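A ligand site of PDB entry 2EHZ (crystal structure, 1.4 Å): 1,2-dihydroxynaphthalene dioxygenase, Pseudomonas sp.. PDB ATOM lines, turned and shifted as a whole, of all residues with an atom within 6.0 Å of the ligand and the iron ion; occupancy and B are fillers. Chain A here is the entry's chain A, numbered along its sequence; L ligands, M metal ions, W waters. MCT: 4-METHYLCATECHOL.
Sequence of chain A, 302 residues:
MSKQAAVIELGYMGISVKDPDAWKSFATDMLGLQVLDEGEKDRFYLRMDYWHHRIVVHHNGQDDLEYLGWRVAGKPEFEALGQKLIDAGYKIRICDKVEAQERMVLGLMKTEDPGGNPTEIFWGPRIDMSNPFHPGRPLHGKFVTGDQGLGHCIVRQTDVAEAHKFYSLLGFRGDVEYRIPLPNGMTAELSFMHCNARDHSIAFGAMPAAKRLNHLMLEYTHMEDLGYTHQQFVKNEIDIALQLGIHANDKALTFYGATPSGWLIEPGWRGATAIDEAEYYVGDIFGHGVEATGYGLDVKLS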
ATOM      1  N   HIS A 152      -6.658  17.546  17.858  1.00  0.00           N
ATOM      2  CA  HIS A 152      -6.248  16.953  16.578  1.00  0.00           C
ATOM      3  C   HIS A 152      -7.412  16.864  15.616  1.00  0.00           C
ATOM      4  O   HIS A 152      -8.566  16.906  16.040  1.00  0.00           O
ATOM      5  CB  HIS A 152      -5.578  15.575  16.743  1.00  0.00           C
ATOM      6  CG  HIS A 152      -6.497  14.439  17.113  1.00  0.00           C
ATOM      7  ND1 HIS A 152      -6.420  13.814  18.334  1.00  0.00           N
ATOM      8  CD2 HIS A 152      -7.438  13.764  16.409  1.00  0.00           C
ATOM      9  CE1 HIS A 152      -7.295  12.823  18.378  1.00  0.00           C
ATOM     10  NE2 HIS A 152      -7.924  12.774  17.215  1.00  0.00           N
ATOM     11  N   ILE A 154      -8.709  14.494  11.990  1.00  0.00           N
ATOM     12  CA  ILE A 154      -8.565  13.675  10.787  1.00  0.00           C
ATOM     13  C   ILE A 154      -9.149  14.463   9.634  1.00  0.00           C
ATOM     14  O   ILE A 154     -10.276  14.965   9.722  1.00  0.00           O
ATOM     15  CB  ILE A 154      -9.245  12.292  10.895  1.00  0.00           C
ATOM     16  CG1 ILE A 154      -8.417  11.384  11.809  1.00  0.00           C
ATOM     17  CG2 ILE A 154      -9.418  11.641   9.505  1.00  0.00           C
ATOM     18  CD1 ILE A 154      -8.869   9.927  11.792  1.00  0.00           C
ATOM     19  N   TYR A 178      -2.616   2.094  12.071  1.00  0.00           N
ATOM     20  CA  TYR A 178      -3.710   1.130  12.089  1.00  0.00           C
ATOM     21  C   TYR A 178      -3.886   0.485  10.744  1.00  0.00           C
ATOM     22  O   TYR A 178      -3.880   1.163   9.710  1.00  0.00           O
ATOM     23  CB  TYR A 178      -5.026   1.789  12.460  1.00  0.00           C
ATOM     24  CG  TYR A 178      -5.117   2.199  13.902  1.00  0.00           C
ATOM     25  CD1 TYR A 178      -4.487   3.342  14.361  1.00  0.00           C
ATOM     26  CD2 TYR A 178      -5.860   1.444  14.812  1.00  0.00           C
ATOM     27  CE1 TYR A 178      -4.577   3.746  15.700  1.00  0.00           C
ATOM     28  CE2 TYR A 178      -5.959   1.838  16.157  1.00  0.00           C
ATOM     29  CZ  TYR A 178      -5.318   2.971  16.575  1.00  0.00           C
ATOM     30  OH  TYR A 178      -5.428   3.369  17.891  1.00  0.00           O
ATOM     31  N   ILE A 180      -6.921  -1.644   9.685  1.00  0.00           N
ATOM     32  CA  ILE A 180      -8.240  -2.042  10.199  1.00  0.00           C
ATOM     33  C   ILE A 180      -9.031  -2.804   9.136  1.00  0.00           C
ATOM     34  O   ILE A 180      -9.245  -2.285   8.043  1.00  0.00           O
ATOM     35  CB  ILE A 180      -9.047  -0.815  10.710  1.00  0.00           C
ATOM     36  CG1 ILE A 180      -8.326  -0.150  11.891  1.00  0.00           C
ATOM     37  CG2 ILE A 180     -10.484  -1.218  11.107  1.00  0.00           C
ATOM     38  CD1 ILE A 180      -8.856   1.227  12.273  1.00  0.00           C
ATOM     39  N   LEU A 190      -4.561   3.757   8.314  1.00  0.00           N
ATOM     40  CA  LEU A 190      -4.656   5.114   8.843  1.00  0.00           C
ATOM     41  C   LEU A 190      -3.312   5.556   9.392  1.00  0.00           C
ATOM     42  O   LEU A 190      -2.666   4.800  10.128  1.00  0.00           O
ATOM     43  CB  LEU A 190      -5.721   5.212   9.934  1.00  0.00           C
ATOM     44  CG  LEU A 190      -7.162   4.886   9.527  1.00  0.00           C
ATOM     45  CD1 LEU A 190      -8.085   5.057  10.713  1.00  0.00           C
ATOM     46  CD2 LEU A 190      -7.632   5.748   8.354  1.00  0.00           C
ATOM     47  N   PHE A 192      -0.937   8.598  11.354  1.00  0.00           N
ATOM     48  CA  PHE A 192      -1.079   9.545  12.468  1.00  0.00           C
ATOM     49  C   PHE A 192       0.242  10.244  12.687  1.00  0.00           C
ATOM     50  O   PHE A 192       1.271   9.590  12.829  1.00  0.00           O
ATOM     51  CB  PHE A 192      -1.474   8.821  13.762  1.00  0.00           C
ATOM     52  CG  PHE A 192      -2.819   8.164  13.697  1.00  0.00           C
ATOM     53  CD1 PHE A 192      -2.994   6.961  13.025  1.00  0.00           C
ATOM     54  CD2 PHE A 192      -3.935   8.765  14.283  1.00  0.00           C
ATOM     55  CE1 PHE A 192      -4.249   6.363  12.947  1.00  0.00           C
ATOM     56  CE2 PHE A 192      -5.190   8.167  14.205  1.00  0.00           C
ATOM     57  CZ  PHE A 192      -5.349   6.969  13.531  1.00  0.00           C
ATOM     58  N   HIS A 200      -1.145  12.565  18.557  1.00  0.00           N
ATOM     59  CA  HIS A 200      -1.227  12.983  17.162  1.00  0.00           C
ATOM     60  C   HIS A 200      -1.929  14.326  17.089  1.00  0.00           C
ATOM     61  O   HIS A 200      -2.774  14.624  17.929  1.00  0.00           O
ATOM     62  CB  HIS A 200      -1.914  11.947  16.262  1.00  0.00           C
ATOM     63  CG  HIS A 200      -3.180  11.350  16.835  1.00  0.00           C
ATOM     64  ND1 HIS A 200      -3.153  10.431  17.855  1.00  0.00           N
ATOM     65  CD2 HIS A 200      -4.481  11.520  16.517  1.00  0.00           C
ATOM     66  CE1 HIS A 200      -4.382  10.065  18.159  1.00  0.00           C
ATOM     67  NE2 HIS A 200      -5.216  10.710  17.355  1.00  0.00           N
ATOM     68  N   HIS A 215     -13.178  14.561  11.727  1.00  0.00           N
ATOM     69  CA  HIS A 215     -13.470  14.908  13.114  1.00  0.00           C
ATOM     70  C   HIS A 215     -12.413  15.806  13.711  1.00  0.00           C
ATOM     71  O   HIS A 215     -11.266  15.829  13.249  1.00  0.00           O
ATOM     72  CB  HIS A 215     -13.686  13.661  14.000  1.00  0.00           C
ATOM     73  CG  HIS A 215     -12.431  12.919  14.342  1.00  0.00           C
ATOM     74  ND1 HIS A 215     -11.901  11.935  13.530  1.00  0.00           N
ATOM     75  CD2 HIS A 215     -11.624  12.989  15.428  1.00  0.00           C
ATOM     76  CE1 HIS A 215     -10.819  11.447  14.102  1.00  0.00           C
ATOM     77  NE2 HIS A 215     -10.626  12.055  15.256  1.00  0.00           N
ATOM     78  N   MET A 217     -10.849  16.431  17.619  1.00  0.00           N
ATOM     79  CA  MET A 217     -10.780  15.906  18.978  1.00  0.00           C
ATOM     80  C   MET A 217     -10.374  17.031  19.911  1.00  0.00           C
ATOM     81  O   MET A 217      -9.388  17.734  19.645  1.00  0.00           O
ATOM     82  CB  MET A 217      -9.750  14.763  19.058  1.00  0.00           C
ATOM     83  CG  MET A 217      -9.701  14.017  20.379  1.00  0.00           C
ATOM     84  SD  MET A 217      -8.627  14.786  21.608  1.00  0.00           S
ATOM     85  CE  MET A 217      -8.843  13.621  22.961  1.00  0.00           C
ATOM     86  N   HIS A 247      -8.416   4.331  22.528  1.00  0.00           N
ATOM     87  CA  HIS A 247      -7.519   4.166  21.386  1.00  0.00           C
ATOM     88  C   HIS A 247      -6.241   3.417  21.750  1.00  0.00           C
ATOM     89  O   HIS A 247      -5.639   3.689  22.791  1.00  0.00           O
ATOM     90  CB  HIS A 247      -7.111   5.521  20.831  1.00  0.00           C
ATOM     91  CG  HIS A 247      -8.220   6.255  20.141  1.00  0.00           C
ATOM     92  ND1 HIS A 247      -8.940   5.700  19.094  1.00  0.00           N
ATOM     93  CD2 HIS A 247      -8.698   7.510  20.302  1.00  0.00           C
ATOM     94  CE1 HIS A 247      -9.813   6.586  18.663  1.00  0.00           C
ATOM     95  NE2 HIS A 247      -9.687   7.692  19.372  1.00  0.00           N
ATOM     96  N   ALA A 248      -5.803   2.516  20.862  1.00  0.00           N
ATOM     97  CA  ALA A 248      -4.526   1.820  21.064  1.00  0.00           C
ATOM     98  C   ALA A 248      -3.314   2.749  20.975  1.00  0.00           C
ATOM     99  O   ALA A 248      -2.349   2.563  21.710  1.00  0.00           O
ATOM    100  CB  ALA A 248      -4.392   0.653  20.101  1.00  0.00           C
ATOM    101  N   ASN A 249      -3.352   3.759  20.090  1.00  0.00           N
ATOM    102  CA  ASN A 249      -2.205   4.660  19.997  1.00  0.00           C
ATOM    103  C   ASN A 249      -2.067   5.651  21.157  1.00  0.00           C
ATOM    104  O   ASN A 249      -1.046   5.632  21.848  1.00  0.00           O
ATOM    105  CB  ASN A 249      -2.074   5.353  18.609  1.00  0.00           C
ATOM    106  CG  ASN A 249      -3.287   6.198  18.193  1.00  0.00           C
ATOM    107  OD1 ASN A 249      -4.253   6.384  18.952  1.00  0.00           O
ATOM    108  ND2 ASN A 249      -3.223   6.733  16.982  1.00  0.00           N
ATOM    109  N   ASP A 250      -3.074   6.470  21.394  1.00  0.00           N
ATOM    110  CA  ASP A 250      -2.922   7.505  22.399  1.00  0.00           C
ATOM    111  C   ASP A 250      -3.498   7.168  23.772  1.00  0.00           C
ATOM    112  O   ASP A 250      -3.356   7.956  24.706  1.00  0.00           O
ATOM    113  CB  ASP A 250      -3.415   8.862  21.912  1.00  0.00           C
ATOM    114  CG  ASP A 250      -4.915   8.951  21.786  1.00  0.00           C
ATOM    115  OD1 ASP A 250      -5.621   7.958  22.085  1.00  0.00           O
ATOM    116  OD2 ASP A 250      -5.383  10.026  21.365  1.00  0.00           O
ATOM    117  N   TYR A 256     -17.350   9.658  19.694  1.00  0.00           N
ATOM    118  CA  TYR A 256     -17.515  10.557  18.556  1.00  0.00           C
ATOM    119  C   TYR A 256     -18.992  10.899  18.383  1.00  0.00           C
ATOM    120  O   TYR A 256     -19.812   9.995  18.176  1.00  0.00           O
ATOM    121  CB  TYR A 256     -17.015   9.889  17.275  1.00  0.00           C
ATOM    122  CG  TYR A 256     -15.548   9.503  17.220  1.00  0.00           C
ATOM    123  CD1 TYR A 256     -15.034   8.446  17.984  1.00  0.00           C
ATOM    124  CD2 TYR A 256     -14.682  10.148  16.329  1.00  0.00           C
ATOM    125  CE1 TYR A 256     -13.700   8.070  17.875  1.00  0.00           C
ATOM    126  CE2 TYR A 256     -13.352   9.786  16.220  1.00  0.00           C
ATOM    127  CZ  TYR A 256     -12.871   8.733  16.980  1.00  0.00           C
ATOM    128  OH  TYR A 256     -11.557   8.329  16.879  1.00  0.00           O
ATOM    129  N   GLU A 266     -14.898  14.690  18.678  1.00  0.00           N
ATOM    130  CA  GLU A 266     -14.422  13.582  19.494  1.00  0.00           C
ATOM    131  C   GLU A 266     -13.981  14.133  20.866  1.00  0.00           C
ATOM    132  O   GLU A 266     -12.813  14.472  21.047  1.00  0.00           O
ATOM    133  CB  GLU A 266     -13.250  12.852  18.789  1.00  0.00           C
ATOM    134  CG  GLU A 266     -12.755  11.626  19.560  1.00  0.00           C
ATOM    135  CD  GLU A 266     -11.477  11.016  19.020  1.00  0.00           C
ATOM    136  OE1 GLU A 266     -10.800  11.622  18.174  1.00  0.00           O
ATOM    137  OE2 GLU A 266     -11.142   9.899  19.491  1.00  0.00           O
ATOM    138  N   ASP A 284      -8.571  -0.922  18.168  1.00  0.00           N
ATOM    139  CA  ASP A 284      -8.434  -0.192  19.429  1.00  0.00           C
ATOM    140  C   ASP A 284      -8.446  -1.164  20.624  1.00  0.00           C
ATOM    141  O   ASP A 284      -8.605  -2.377  20.457  1.00  0.00           O
ATOM    142  CB  ASP A 284      -9.528   0.898  19.523  1.00  0.00           C
ATOM    143  CG  ASP A 284      -9.082   2.243  18.951  1.00  0.00           C
ATOM    144  OD1 ASP A 284      -7.863   2.463  18.764  1.00  0.00           O
ATOM    145  OD2 ASP A 284      -9.943   3.123  18.729  1.00  0.00           O
ATOM    146  N   LEU A 297     -17.460   8.253   9.947  1.00  0.00           N
ATOM    147  CA  LEU A 297     -16.976   6.968  10.441  1.00  0.00           C
ATOM    148  C   LEU A 297     -18.125   5.977  10.586  1.00  0.00           C
ATOM    149  O   LEU A 297     -18.945   6.081  11.506  1.00  0.00           O
ATOM    150  CB  LEU A 297     -16.217   7.153  11.761  1.00  0.00           C
ATOM    151  CG  LEU A 297     -15.032   8.131  11.723  1.00  0.00           C
ATOM    152  CD1 LEU A 297     -14.656   8.571  13.122  1.00  0.00           C
ATOM    153  CD2 LEU A 297     -13.829   7.545  11.002  1.00  0.00           C
ATOM    154  N   LEU A 301     -13.899   0.461  15.268  1.00  0.00           N
ATOM    155  CA  LEU A 301     -12.449   0.594  15.420  1.00  0.00           C
ATOM    156  C   LEU A 301     -11.809  -0.528  16.236  1.00  0.00           C
ATOM    157  O   LEU A 301     -10.577  -0.605  16.309  1.00  0.00           O
ATOM    158  CB  LEU A 301     -12.076   1.965  16.005  1.00  0.00           C
ATOM    159  CG  LEU A 301     -12.419   3.212  15.190  1.00  0.00           C
ATOM    160  CD1 LEU A 301     -11.881   4.456  15.881  1.00  0.00           C
ATOM    161  CD2 LEU A 301     -11.879   3.122  13.758  1.00  0.00           C
HETATM  162  C1  MCT L   1      -7.972   6.169  15.721  1.00  0.00           C
HETATM  163  C2  MCT L   1      -8.834   7.191  15.375  1.00  0.00           C
HETATM  164  C3  MCT L   1      -8.710   8.423  16.004  1.00  0.00           C
HETATM  165  O3  MCT L   1      -9.573   9.438  15.679  1.00  0.00           O
HETATM  166  C4  MCT L   1      -7.749   8.648  16.968  1.00  0.00           C
HETATM  167  O4  MCT L   1      -7.684   9.892  17.546  1.00  0.00           O
HETATM  168  C5  MCT L   1      -6.859   7.627  17.339  1.00  0.00           C
HETATM  169  C6  MCT L   1      -6.994   6.384  16.691  1.00  0.00           C
HETATM  170  C   MCT L   1      -8.108   4.822  15.043  1.00  0.00           C
HETATM  171 FE    FE M   1      -9.355  11.175  16.806  1.00  0.00          FE
HETATM  172  O   HOH W   1      -8.011  10.619  20.590  1.00  0.00           O
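A ring nitrogen (NE2) of His 247 sits close to an oxygen (O4) of the ligand (3.5 Å).
An oxygen (O3) of the ligand sits close to the side-chain hydroxyl (OH) of Tyr 256, at 2.6 Å.
NE2 of His 200 lies close to O4 of the ligand (2.6 Å).
O of His 152 sits at hydrogen-bond distance from N of Met 217 (2.8 Å).
The backbone carbonyl oxygen (O) of His 215 sits at hydrogen-bond distance from the backbone NH (N) of Ile 154, 3.1 Å away.
The side-chain carboxylate of Asp 284 sits at hydrogen-bond distance from the side-chain hydroxyl of Tyr 178, at 2.7 Å.
N of Ala 248 is in hydrogen-bond range of OH of Tyr 178.
A ring nitrogen (ND1) of His 247 lies within hydrogen-bond range of the side-chain carboxylate of Asp 284 (2.8 Å).
The side-chain hydroxyl (OH) of Tyr 256 lies close to a ring nitrogen (NE2) of His 247 (3.2 Å).
N of Asp 284 is in hydrogen-bond range of O of Leu 301, 2.8 Å away.
A ring nitrogen (NE2) of His 200 sits close to a ring nitrogen (ND1) of His 152, 3.5 Å away.
Residues that only touch the ligand: Asn 249 (3.3 Å), Phe 192 (3.5 Å), Tyr 178 (3.6 Å), Leu 301 (3.9 Å) and Ile 154 (3.98 Å).
Of the 18 residues printed, 11 come within 4 Å of the ligand.
Along chain A the residues within 4 Å of the ligand span positions 152 to 301.
Merely in contact with the iron ion: Tyr 256.
Within 4 Å of the iron ion: His 152, His 215, Tyr 256 and Glu 266.
The iron ion is bound by OE1 of Glu 266 (2.0 Å), O3 of the ligand (2.1 Å), NE2 of His 152 (2.2 Å), NE2 of His 215 (2.2 Å) and O4 of the ligand (2.2 Å).
Water W1 lies within hydrogen-bond range of OD2 of Asp 250 (2.8 Å) and OE2 of Glu 266 (3.4 Å).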
